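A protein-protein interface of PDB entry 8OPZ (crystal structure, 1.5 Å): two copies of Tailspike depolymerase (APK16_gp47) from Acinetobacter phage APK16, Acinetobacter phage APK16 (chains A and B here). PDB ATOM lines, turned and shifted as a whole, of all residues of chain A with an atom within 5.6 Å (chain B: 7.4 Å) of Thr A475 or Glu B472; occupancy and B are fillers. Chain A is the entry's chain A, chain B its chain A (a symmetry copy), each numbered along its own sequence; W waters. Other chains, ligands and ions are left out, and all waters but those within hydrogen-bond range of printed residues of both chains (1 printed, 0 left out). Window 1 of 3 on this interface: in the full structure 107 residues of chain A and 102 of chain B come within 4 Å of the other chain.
Of chain B, only Ile B470 and Glu B472 come within 4 Å of Thr A475.
Of chain A, only Lys A451 (3.4 Å) and Thr A475 (2.8 Å) come within 4 Å of Glu B472.
Of the printed residues of chain B, Asn A504 touches Ile B470 (3.6 Å) and Ile B499 (3.8 Å).
Of the printed residues of chain A, Ile B470 touches Thr A475 (3.6 Å), Ile A477 (3.8 Å) and Asn A504 (3.6 Å).
Of the printed residues of chain A, Ile B447 touches Lys A451 (3.9 Å) and Ile A477 (3.7 Å).
The nearest residue of chain B that does not touch Thr A475 is Ile B447 (4.1 Å).
The nearest residue of chain A that does not touch Glu B472 is Asn A504 (4.03 Å).
Positions printed for both chains: 450, 473, 474, 502 and 504.
Of the 8 pairs that touch across the chains among the printed residues, none has its exchanged pair printed and touching as well.
Ile B447 touches Lys A451.
Thr A475 touches Ile B470.
Ile A477 touches Ile B447.
Ile A477 touches Ile B470 (CG1 to CD1, 3.8 Å).
CG of Asn A504 touches CG2 of Ile B470, at 3.6 Å.
Ile B499 touches Asn A504 (CG2 to OD1, 3.8 Å).
The side-chain carboxylate (OE2) of Glu B472 sits at hydrogen-bond distance from the side-chain hydroxyl (OG1) of Thr A475.
The side-chain amino group of Lys A451 lies within salt-bridge range of the side-chain carboxylate of Glu B472, 3.4 Å away.
Of the 20 printed residues of chain B, 4 touch a printed residue of chain A.
Printed residues of chain B that touch a printed residue of chain A: Ile B447, Ile B470, Glu B472 and Ile B499.
Hydrophobic or aromatic side chains of chain B within 4 Å of the printed part of chain A: Ile B447, Ile B470 and Ile B499.
Of the 12 printed residues of chain A, 4 touch a printed residue of chain B.
Printed residues of chain A that touch a printed residue of chain B: Lys A451, Thr A475, Ile A477 and Asn A504.
Hydrophobic or aromatic side chains of chain A within 4 Å of the printed part of chain B: Ile A477.
Among the printed residues, 8 pairs touch across the chains.
Water W1 lies within hydrogen-bond range of the backbone carbonyl oxygen (O) of Ala A450 (2.8 Å), the side-chain carboxylate (OE2) of Glu B472 (3.0 Å) and the side-chain amino group (NZ) of Lys A451 (3.1 Å).
The side-chain hydroxyl of Thr A475 lies within hydrogen-bond range of the side-chain amide nitrogen of Asn A504 (2.8 Å).
The backbone NH of Val B448 lies within hydrogen-bond range of the backbone carbonyl oxygen of Ile B470.
N of Val B471 sits at hydrogen-bond distance from O of Ile B499, 2.7 Å away.
O of Ser B469 sits at hydrogen-bond distance from N of Ile B499.
The backbone NH of Val B430 lies within hydrogen-bond range of the backbone carbonyl oxygen of Ile B447 (2.7 Å).
The backbone carbonyl oxygen (O) of Glu B472 is in hydrogen-bond range of the backbone NH (N) of Arg B502.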
ATOM      1  N   ALA A 450      10.814 -23.267 -17.145  1.00  0.00           N
ATOM      2  CA  ALA A 450      10.836 -24.420 -18.071  1.00  0.00           C
ATOM      3  C   ALA A 450      11.398 -25.690 -17.478  1.00  0.00           C
ATOM      4  O   ALA A 450      12.359 -25.641 -16.677  1.00  0.00           O
ATOM      5  CB  ALA A 450      11.525 -24.070 -19.338  1.00  0.00           C
ATOM      6  N   LYS A 451      10.770 -26.823 -17.915  1.00  0.00           N
ATOM      7  CA  LYS A 451      11.319 -28.177 -17.686  1.00  0.00           C
ATOM      8  C   LYS A 451      11.327 -28.804 -19.093  1.00  0.00           C
ATOM      9  O   LYS A 451      10.280 -29.018 -19.717  1.00  0.00           O
ATOM     10  CB  LYS A 451      10.703 -29.072 -16.594  1.00  0.00           C
ATOM     11  CG  LYS A 451      10.655 -28.352 -15.274  1.00  0.00           C
ATOM     12  CD  LYS A 451       9.461 -28.716 -14.518  1.00  0.00           C
ATOM     13  CE  LYS A 451       9.296 -28.099 -13.135  1.00  0.00           C
ATOM     14  NZ  LYS A 451       9.054 -26.641 -13.283  1.00  0.00           N
ATOM     15  N   ILE A 452      12.533 -29.012 -19.656  1.00  0.00           N
ATOM     16  CA  ILE A 452      12.701 -29.559 -21.019  1.00  0.00           C
ATOM     17  C   ILE A 452      13.621 -30.788 -20.986  1.00  0.00           C
ATOM     18  O   ILE A 452      14.760 -30.692 -20.468  1.00  0.00           O
ATOM     19  CB  ILE A 452      13.080 -28.475 -22.096  1.00  0.00           C
ATOM     20  CG1 ILE A 452      12.233 -27.171 -22.094  1.00  0.00           C
ATOM     21  CG2 ILE A 452      13.344 -29.002 -23.506  1.00  0.00           C
ATOM     22  CD1 ILE A 452      10.762 -27.258 -22.339  1.00  0.00           C
ATOM     23  N   THR A 453      13.108 -31.877 -21.628  1.00  0.00           N
ATOM     24  CA  THR A 453      13.746 -33.201 -21.824  1.00  0.00           C
ATOM     25  C   THR A 453      14.026 -33.423 -23.317  1.00  0.00           C
ATOM     26  O   THR A 453      13.102 -33.209 -24.122  1.00  0.00           O
ATOM     27  CB  THR A 453      13.046 -34.314 -21.014  1.00  0.00           C
ATOM     28  OG1 THR A 453      12.970 -33.828 -19.667  1.00  0.00           O
ATOM     29  CG2 THR A 453      13.760 -35.655 -20.976  1.00  0.00           C
ATOM     30  N   ALA A 459      17.581 -26.169 -24.805  1.00  0.00           N
ATOM     31  CA  ALA A 459      16.279 -26.214 -24.133  1.00  0.00           C
ATOM     32  C   ALA A 459      15.512 -24.895 -24.366  1.00  0.00           C
ATOM     33  O   ALA A 459      14.411 -24.910 -24.949  1.00  0.00           O
ATOM     34  CB  ALA A 459      16.414 -26.716 -22.718  1.00  0.00           C
ATOM     35  N   GLU A 473      13.613 -20.243 -13.577  1.00  0.00           N
ATOM     36  CA  GLU A 473      14.119 -21.602 -13.530  1.00  0.00           C
ATOM     37  C   GLU A 473      14.000 -22.265 -14.898  1.00  0.00           C
ATOM     38  O   GLU A 473      12.943 -22.147 -15.546  1.00  0.00           O
ATOM     39  CB  GLU A 473      13.363 -22.430 -12.480  1.00  0.00           C
ATOM     40  N   VAL A 474      15.111 -22.901 -15.295  1.00  0.00           N
ATOM     41  CA  VAL A 474      15.138 -23.833 -16.431  1.00  0.00           C
ATOM     42  C   VAL A 474      15.833 -25.144 -15.983  1.00  0.00           C
ATOM     43  O   VAL A 474      16.961 -25.111 -15.435  1.00  0.00           O
ATOM     44  CB  VAL A 474      15.709 -23.250 -17.742  1.00  0.00           C
ATOM     45  CG1 VAL A 474      15.850 -24.245 -18.862  1.00  0.00           C
ATOM     46  CG2 VAL A 474      15.044 -21.988 -18.275  1.00  0.00           C
ATOM     47  N   THR A 475      15.012 -26.209 -16.031  1.00  0.00           N
ATOM     48  CA  THR A 475      15.532 -27.534 -15.818  1.00  0.00           C
ATOM     49  C   THR A 475      15.608 -28.202 -17.196  1.00  0.00           C
ATOM     50  O   THR A 475      14.569 -28.419 -17.837  1.00  0.00           O
ATOM     51  CB  THR A 475      14.786 -28.189 -14.656  1.00  0.00           C
ATOM     52  OG1 THR A 475      15.032 -27.438 -13.442  1.00  0.00           O
ATOM     53  CG2 THR A 475      15.413 -29.522 -14.462  1.00  0.00           C
ATOM     54  N   ALA A 476      16.842 -28.710 -17.469  1.00  0.00           N
ATOM     55  CA  ALA A 476      17.123 -29.400 -18.728  1.00  0.00           C
ATOM     56  C   ALA A 476      17.740 -30.759 -18.409  1.00  0.00           C
ATOM     57  O   ALA A 476      18.881 -30.868 -17.925  1.00  0.00           O
ATOM     58  CB  ALA A 476      17.921 -28.578 -19.748  1.00  0.00           C
ATOM     59  N   ILE A 477      17.026 -31.757 -18.917  1.00  0.00           N
ATOM     60  CA  ILE A 477      17.514 -33.122 -18.937  1.00  0.00           C
ATOM     61  C   ILE A 477      17.872 -33.542 -20.389  1.00  0.00           C
ATOM     62  O   ILE A 477      17.037 -33.501 -21.318  1.00  0.00           O
ATOM     63  CB  ILE A 477      16.542 -34.075 -18.173  1.00  0.00           C
ATOM     64  CG1 ILE A 477      16.126 -33.621 -16.754  1.00  0.00           C
ATOM     65  CG2 ILE A 477      17.021 -35.532 -18.221  1.00  0.00           C
ATOM     66  CD1 ILE A 477      14.853 -34.228 -16.192  1.00  0.00           C
ATOM     67  N   ARG A 502      17.969 -19.699 -11.814  1.00  0.00           N
ATOM     68  CA  ARG A 502      18.478 -21.041 -11.587  1.00  0.00           C
ATOM     69  C   ARG A 502      18.293 -21.796 -12.891  1.00  0.00           C
ATOM     70  O   ARG A 502      17.142 -21.939 -13.361  1.00  0.00           O
ATOM     71  CB  ARG A 502      17.883 -21.726 -10.344  1.00  0.00           C
ATOM     72  N   ASN A 504      19.283 -25.534 -14.192  1.00  0.00           N
ATOM     73  CA  ASN A 504      19.492 -26.961 -13.857  1.00  0.00           C
ATOM     74  C   ASN A 504      19.836 -27.775 -15.131  1.00  0.00           C
ATOM     75  O   ASN A 504      19.009 -27.910 -16.012  1.00  0.00           O
ATOM     76  CB  ASN A 504      18.388 -27.585 -12.973  1.00  0.00           C
ATOM     77  CG  ASN A 504      18.050 -26.684 -11.800  1.00  0.00           C
ATOM     78  OD1 ASN A 504      18.885 -26.417 -10.917  1.00  0.00           O
ATOM     79  ND2 ASN A 504      16.849 -26.116 -11.797  1.00  0.00           N
ATOM     80  N   VAL B 430       7.305 -34.252 -10.052  1.00  0.00           N
ATOM     81  CA  VAL B 430       6.636 -34.299  -8.754  1.00  0.00           C
ATOM     82  C   VAL B 430       6.485 -32.886  -8.213  1.00  0.00           C
ATOM     83  O   VAL B 430       7.471 -32.174  -8.135  1.00  0.00           O
ATOM     84  CB  VAL B 430       7.366 -35.248  -7.764  1.00  0.00           C
ATOM     85  CG1 VAL B 430       7.130 -35.028  -6.272  1.00  0.00           C
ATOM     86  CG2 VAL B 430       7.260 -36.734  -8.124  1.00  0.00           C
ATOM     87  N   ASN B 431       5.233 -32.581  -7.944  1.00  0.00           N
ATOM     88  CA  ASN B 431       4.745 -31.371  -7.285  1.00  0.00           C
ATOM     89  C   ASN B 431       3.804 -31.745  -6.114  1.00  0.00           C
ATOM     90  O   ASN B 431       2.721 -32.229  -6.353  1.00  0.00           O
ATOM     91  CB  ASN B 431       4.054 -30.428  -8.281  1.00  0.00           C
ATOM     92  CG  ASN B 431       4.971 -29.513  -9.067  1.00  0.00           C
ATOM     93  OD1 ASN B 431       5.375 -28.466  -8.569  1.00  0.00           O
ATOM     94  ND2 ASN B 431       5.217 -29.847 -10.330  1.00  0.00           N
ATOM     95  N   THR B 446      14.207 -37.448 -11.761  1.00  0.00           N
ATOM     96  CA  THR B 446      12.957 -37.062 -11.041  1.00  0.00           C
ATOM     97  C   THR B 446      13.119 -35.547 -10.818  1.00  0.00           C
ATOM     98  O   THR B 446      14.249 -35.139 -10.412  1.00  0.00           O
ATOM     99  CB  THR B 446      12.610 -37.851  -9.743  1.00  0.00           C
ATOM    100  OG1 THR B 446      12.810 -39.283  -9.767  1.00  0.00           O
ATOM    101  CG2 THR B 446      11.222 -37.485  -9.225  1.00  0.00           C
ATOM    102  N   ILE B 447      12.055 -34.788 -11.228  1.00  0.00           N
ATOM    103  CA  ILE B 447      12.000 -33.367 -10.841  1.00  0.00           C
ATOM    104  C   ILE B 447      11.035 -33.216  -9.642  1.00  0.00           C
ATOM    105  O   ILE B 447       9.871 -33.632  -9.788  1.00  0.00           O
ATOM    106  CB  ILE B 447      11.687 -32.436 -12.058  1.00  0.00           C
ATOM    107  CG1 ILE B 447      12.683 -32.558 -13.238  1.00  0.00           C
ATOM    108  CG2 ILE B 447      11.507 -30.980 -11.622  1.00  0.00           C
ATOM    109  CD1 ILE B 447      12.196 -32.114 -14.658  1.00  0.00           C
ATOM    110  N   VAL B 448      11.582 -32.617  -8.529  1.00  0.00           N
ATOM    111  CA  VAL B 448      10.923 -32.530  -7.216  1.00  0.00           C
ATOM    112  C   VAL B 448      10.609 -31.059  -6.874  1.00  0.00           C
ATOM    113  O   VAL B 448      11.593 -30.327  -6.833  1.00  0.00           O
ATOM    114  CB  VAL B 448      11.696 -33.324  -6.125  1.00  0.00           C
ATOM    115  CG1 VAL B 448      11.032 -33.249  -4.749  1.00  0.00           C
ATOM    116  CG2 VAL B 448      11.932 -34.768  -6.526  1.00  0.00           C
ATOM    117  N   ASN B 449       9.321 -30.800  -6.609  1.00  0.00           N
ATOM    118  CA  ASN B 449       8.949 -29.560  -5.868  1.00  0.00           C
ATOM    119  C   ASN B 449       8.003 -29.987  -4.739  1.00  0.00           C
ATOM    120  O   ASN B 449       6.982 -30.620  -4.963  1.00  0.00           O
ATOM    121  CB  ASN B 449       8.364 -28.441  -6.731  1.00  0.00           C
ATOM    122  CG  ASN B 449       9.442 -27.752  -7.525  1.00  0.00           C
ATOM    123  OD1 ASN B 449      10.193 -26.895  -7.030  1.00  0.00           O
ATOM    124  ND2 ASN B 449       9.584 -28.225  -8.750  1.00  0.00           N
ATOM    125  N   ALA B 450       8.394 -29.497  -3.522  1.00  0.00           N
ATOM    126  CA  ALA B 450       7.589 -29.856  -2.335  1.00  0.00           C
ATOM    127  C   ALA B 450       7.419 -28.739  -1.333  1.00  0.00           C
ATOM    128  O   ALA B 450       8.359 -27.942  -1.110  1.00  0.00           O
ATOM    129  CB  ALA B 450       8.117 -31.082  -1.686  1.00  0.00           C
ATOM    130  N   GLY B 468      20.641 -38.414 -11.812  1.00  0.00           N
ATOM    131  CA  GLY B 468      20.213 -37.243 -12.559  1.00  0.00           C
ATOM    132  C   GLY B 468      18.885 -36.554 -12.180  1.00  0.00           C
ATOM    133  O   GLY B 468      18.378 -35.808 -13.084  1.00  0.00           O
ATOM    134  N   SER B 469      18.404 -36.653 -10.862  1.00  0.00           N
ATOM    135  CA  SER B 469      17.291 -35.995 -10.164  1.00  0.00           C
ATOM    136  C   SER B 469      17.654 -34.547  -9.869  1.00  0.00           C
ATOM    137  O   SER B 469      18.812 -34.229  -9.554  1.00  0.00           O
ATOM    138  CB  SER B 469      16.647 -36.782  -8.946  1.00  0.00           C
ATOM    139  OG  SER B 469      16.040 -37.921  -9.477  1.00  0.00           O
ATOM    140  N   ILE B 470      16.625 -33.713 -10.159  1.00  0.00           N
ATOM    141  CA  ILE B 470      16.713 -32.312  -9.759  1.00  0.00           C
ATOM    142  C   ILE B 470      15.551 -32.059  -8.787  1.00  0.00           C
ATOM    143  O   ILE B 470      14.315 -32.119  -9.049  1.00  0.00           O
ATOM    144  CB  ILE B 470      16.708 -31.335 -10.979  1.00  0.00           C
ATOM    145  CG1 ILE B 470      17.513 -31.721 -12.230  1.00  0.00           C
ATOM    146  CG2 ILE B 470      16.636 -29.835 -10.724  1.00  0.00           C
ATOM    147  CD1 ILE B 470      16.696 -32.625 -13.176  1.00  0.00           C
ATOM    148  N   VAL B 471      16.115 -31.608  -7.647  1.00  0.00           N
ATOM    149  CA  VAL B 471      15.216 -31.228  -6.592  1.00  0.00           C
ATOM    150  C   VAL B 471      15.322 -29.712  -6.658  1.00  0.00           C
ATOM    151  O   VAL B 471      16.333 -29.189  -6.232  1.00  0.00           O
ATOM    152  CB  VAL B 471      15.641 -31.821  -5.229  1.00  0.00           C
ATOM    153  CG1 VAL B 471      14.817 -31.262  -4.078  1.00  0.00           C
ATOM    154  CG2 VAL B 471      15.609 -33.351  -5.102  1.00  0.00           C
ATOM    155  N   GLU B 472      14.269 -29.140  -7.257  1.00  0.00           N
ATOM    156  CA  GLU B 472      14.203 -27.700  -7.463  1.00  0.00           C
ATOM    157  C   GLU B 472      14.067 -26.956  -6.133  1.00  0.00           C
ATOM    158  O   GLU B 472      14.926 -26.191  -5.786  1.00  0.00           O
ATOM    159  CB  GLU B 472      13.121 -27.432  -8.499  1.00  0.00           C
ATOM    160  CG  GLU B 472      13.539 -27.503  -9.973  1.00  0.00           C
ATOM    161  CD  GLU B 472      12.418 -27.277 -10.988  1.00  0.00           C
ATOM    162  OE1 GLU B 472      11.259 -26.757 -10.682  1.00  0.00           O
ATOM    163  OE2 GLU B 472      12.637 -27.788 -12.064  1.00  0.00           O
ATOM    164  N   GLU B 473      12.996 -27.255  -5.394  1.00  0.00           N
ATOM    165  CA  GLU B 473      12.634 -26.601  -4.151  1.00  0.00           C
ATOM    166  C   GLU B 473      11.918 -27.575  -3.221  1.00  0.00           C
ATOM    167  O   GLU B 473      11.023 -28.312  -3.678  1.00  0.00           O
ATOM    168  CB  GLU B 473      11.741 -25.380  -4.416  1.00  0.00           C
ATOM    169  N   VAL B 474      12.375 -27.565  -1.962  1.00  0.00           N
ATOM    170  CA  VAL B 474      11.663 -28.204  -0.845  1.00  0.00           C
ATOM    171  C   VAL B 474      11.551 -27.190   0.320  1.00  0.00           C
ATOM    172  O   VAL B 474      12.572 -26.599   0.750  1.00  0.00           O
ATOM    173  CB  VAL B 474      12.222 -29.578  -0.415  1.00  0.00           C
ATOM    174  CG1 VAL B 474      11.568 -30.166   0.807  1.00  0.00           C
ATOM    175  CG2 VAL B 474      12.315 -30.647  -1.495  1.00  0.00           C
ATOM    176  N   ILE B 499      21.123 -33.031  -8.525  1.00  0.00           N
ATOM    177  CA  ILE B 499      21.071 -31.600  -8.104  1.00  0.00           C
ATOM    178  C   ILE B 499      19.998 -31.428  -7.011  1.00  0.00           C
ATOM    179  O   ILE B 499      18.829 -31.701  -7.230  1.00  0.00           O
ATOM    180  CB  ILE B 499      20.826 -30.621  -9.311  1.00  0.00           C
ATOM    181  CG1 ILE B 499      21.831 -30.718 -10.452  1.00  0.00           C
ATOM    182  CG2 ILE B 499      20.538 -29.189  -8.884  1.00  0.00           C
ATOM    183  CD1 ILE B 499      21.402 -30.332 -11.837  1.00  0.00           C
ATOM    184  N   ILE B 500      20.499 -30.954  -5.843  1.00  0.00           N
ATOM    185  CA  ILE B 500      19.616 -30.502  -4.795  1.00  0.00           C
ATOM    186  C   ILE B 500      19.650 -28.972  -4.826  1.00  0.00           C
ATOM    187  O   ILE B 500      20.701 -28.399  -4.466  1.00  0.00           O
ATOM    188  CB  ILE B 500      19.897 -31.183  -3.430  1.00  0.00           C
ATOM    189  CG1 ILE B 500      20.258 -32.679  -3.368  1.00  0.00           C
ATOM    190  CG2 ILE B 500      18.888 -30.942  -2.389  1.00  0.00           C
ATOM    191  CD1 ILE B 500      19.388 -33.650  -4.037  1.00  0.00           C
ATOM    192  N   GLY B 501      18.510 -28.348  -5.231  1.00  0.00           N
ATOM    193  CA  GLY B 501      18.407 -26.892  -5.327  1.00  0.00           C
ATOM    194  C   GLY B 501      18.162 -26.280  -3.953  1.00  0.00           C
ATOM    195  O   GLY B 501      18.858 -26.598  -2.985  1.00  0.00           O
ATOM    196  N   ARG B 502      17.111 -25.470  -3.890  1.00  0.00           N
ATOM    197  CA  ARG B 502      16.793 -24.659  -2.727  1.00  0.00           C
ATOM    198  C   ARG B 502      15.983 -25.544  -1.797  1.00  0.00           C
ATOM    199  O   ARG B 502      14.895 -26.019  -2.193  1.00  0.00           O
ATOM    200  CB  ARG B 502      16.145 -23.307  -3.074  1.00  0.00           C
ATOM    201  N   ILE B 503      16.579 -25.709  -0.594  1.00  0.00           N
ATOM    202  CA  ILE B 503      15.933 -26.303   0.568  1.00  0.00           C
ATOM    203  C   ILE B 503      15.712 -25.154   1.568  1.00  0.00           C
ATOM    204  O   ILE B 503      16.680 -24.558   2.024  1.00  0.00           O
ATOM    205  CB  ILE B 503      16.805 -27.502   1.069  1.00  0.00           C
ATOM    206  CG1 ILE B 503      17.346 -28.510   0.018  1.00  0.00           C
ATOM    207  CG2 ILE B 503      16.209 -28.222   2.272  1.00  0.00           C
ATOM    208  CD1 ILE B 503      16.325 -29.072  -0.932  1.00  0.00           C
ATOM    209  N   ASN B 504      14.411 -25.077   1.939  1.00  0.00           N
ATOM    210  CA  ASN B 504      13.823 -24.162   2.944  1.00  0.00           C
ATOM    211  C   ASN B 504      13.408 -24.944   4.217  1.00  0.00           C
ATOM    212  O   ASN B 504      12.512 -25.765   4.166  1.00  0.00           O
ATOM    213  CB  ASN B 504      12.739 -23.209   2.392  1.00  0.00           C
ATOM    214  CG  ASN B 504      13.189 -22.553   1.101  1.00  0.00           C
ATOM    215  OD1 ASN B 504      14.168 -21.785   1.064  1.00  0.00           O
ATOM    216  ND2 ASN B 504      12.551 -22.901  -0.012  1.00  0.00           N
HETATM  217  O   HOH W   1      11.900 -25.496 -13.878  1.00  0.00           O
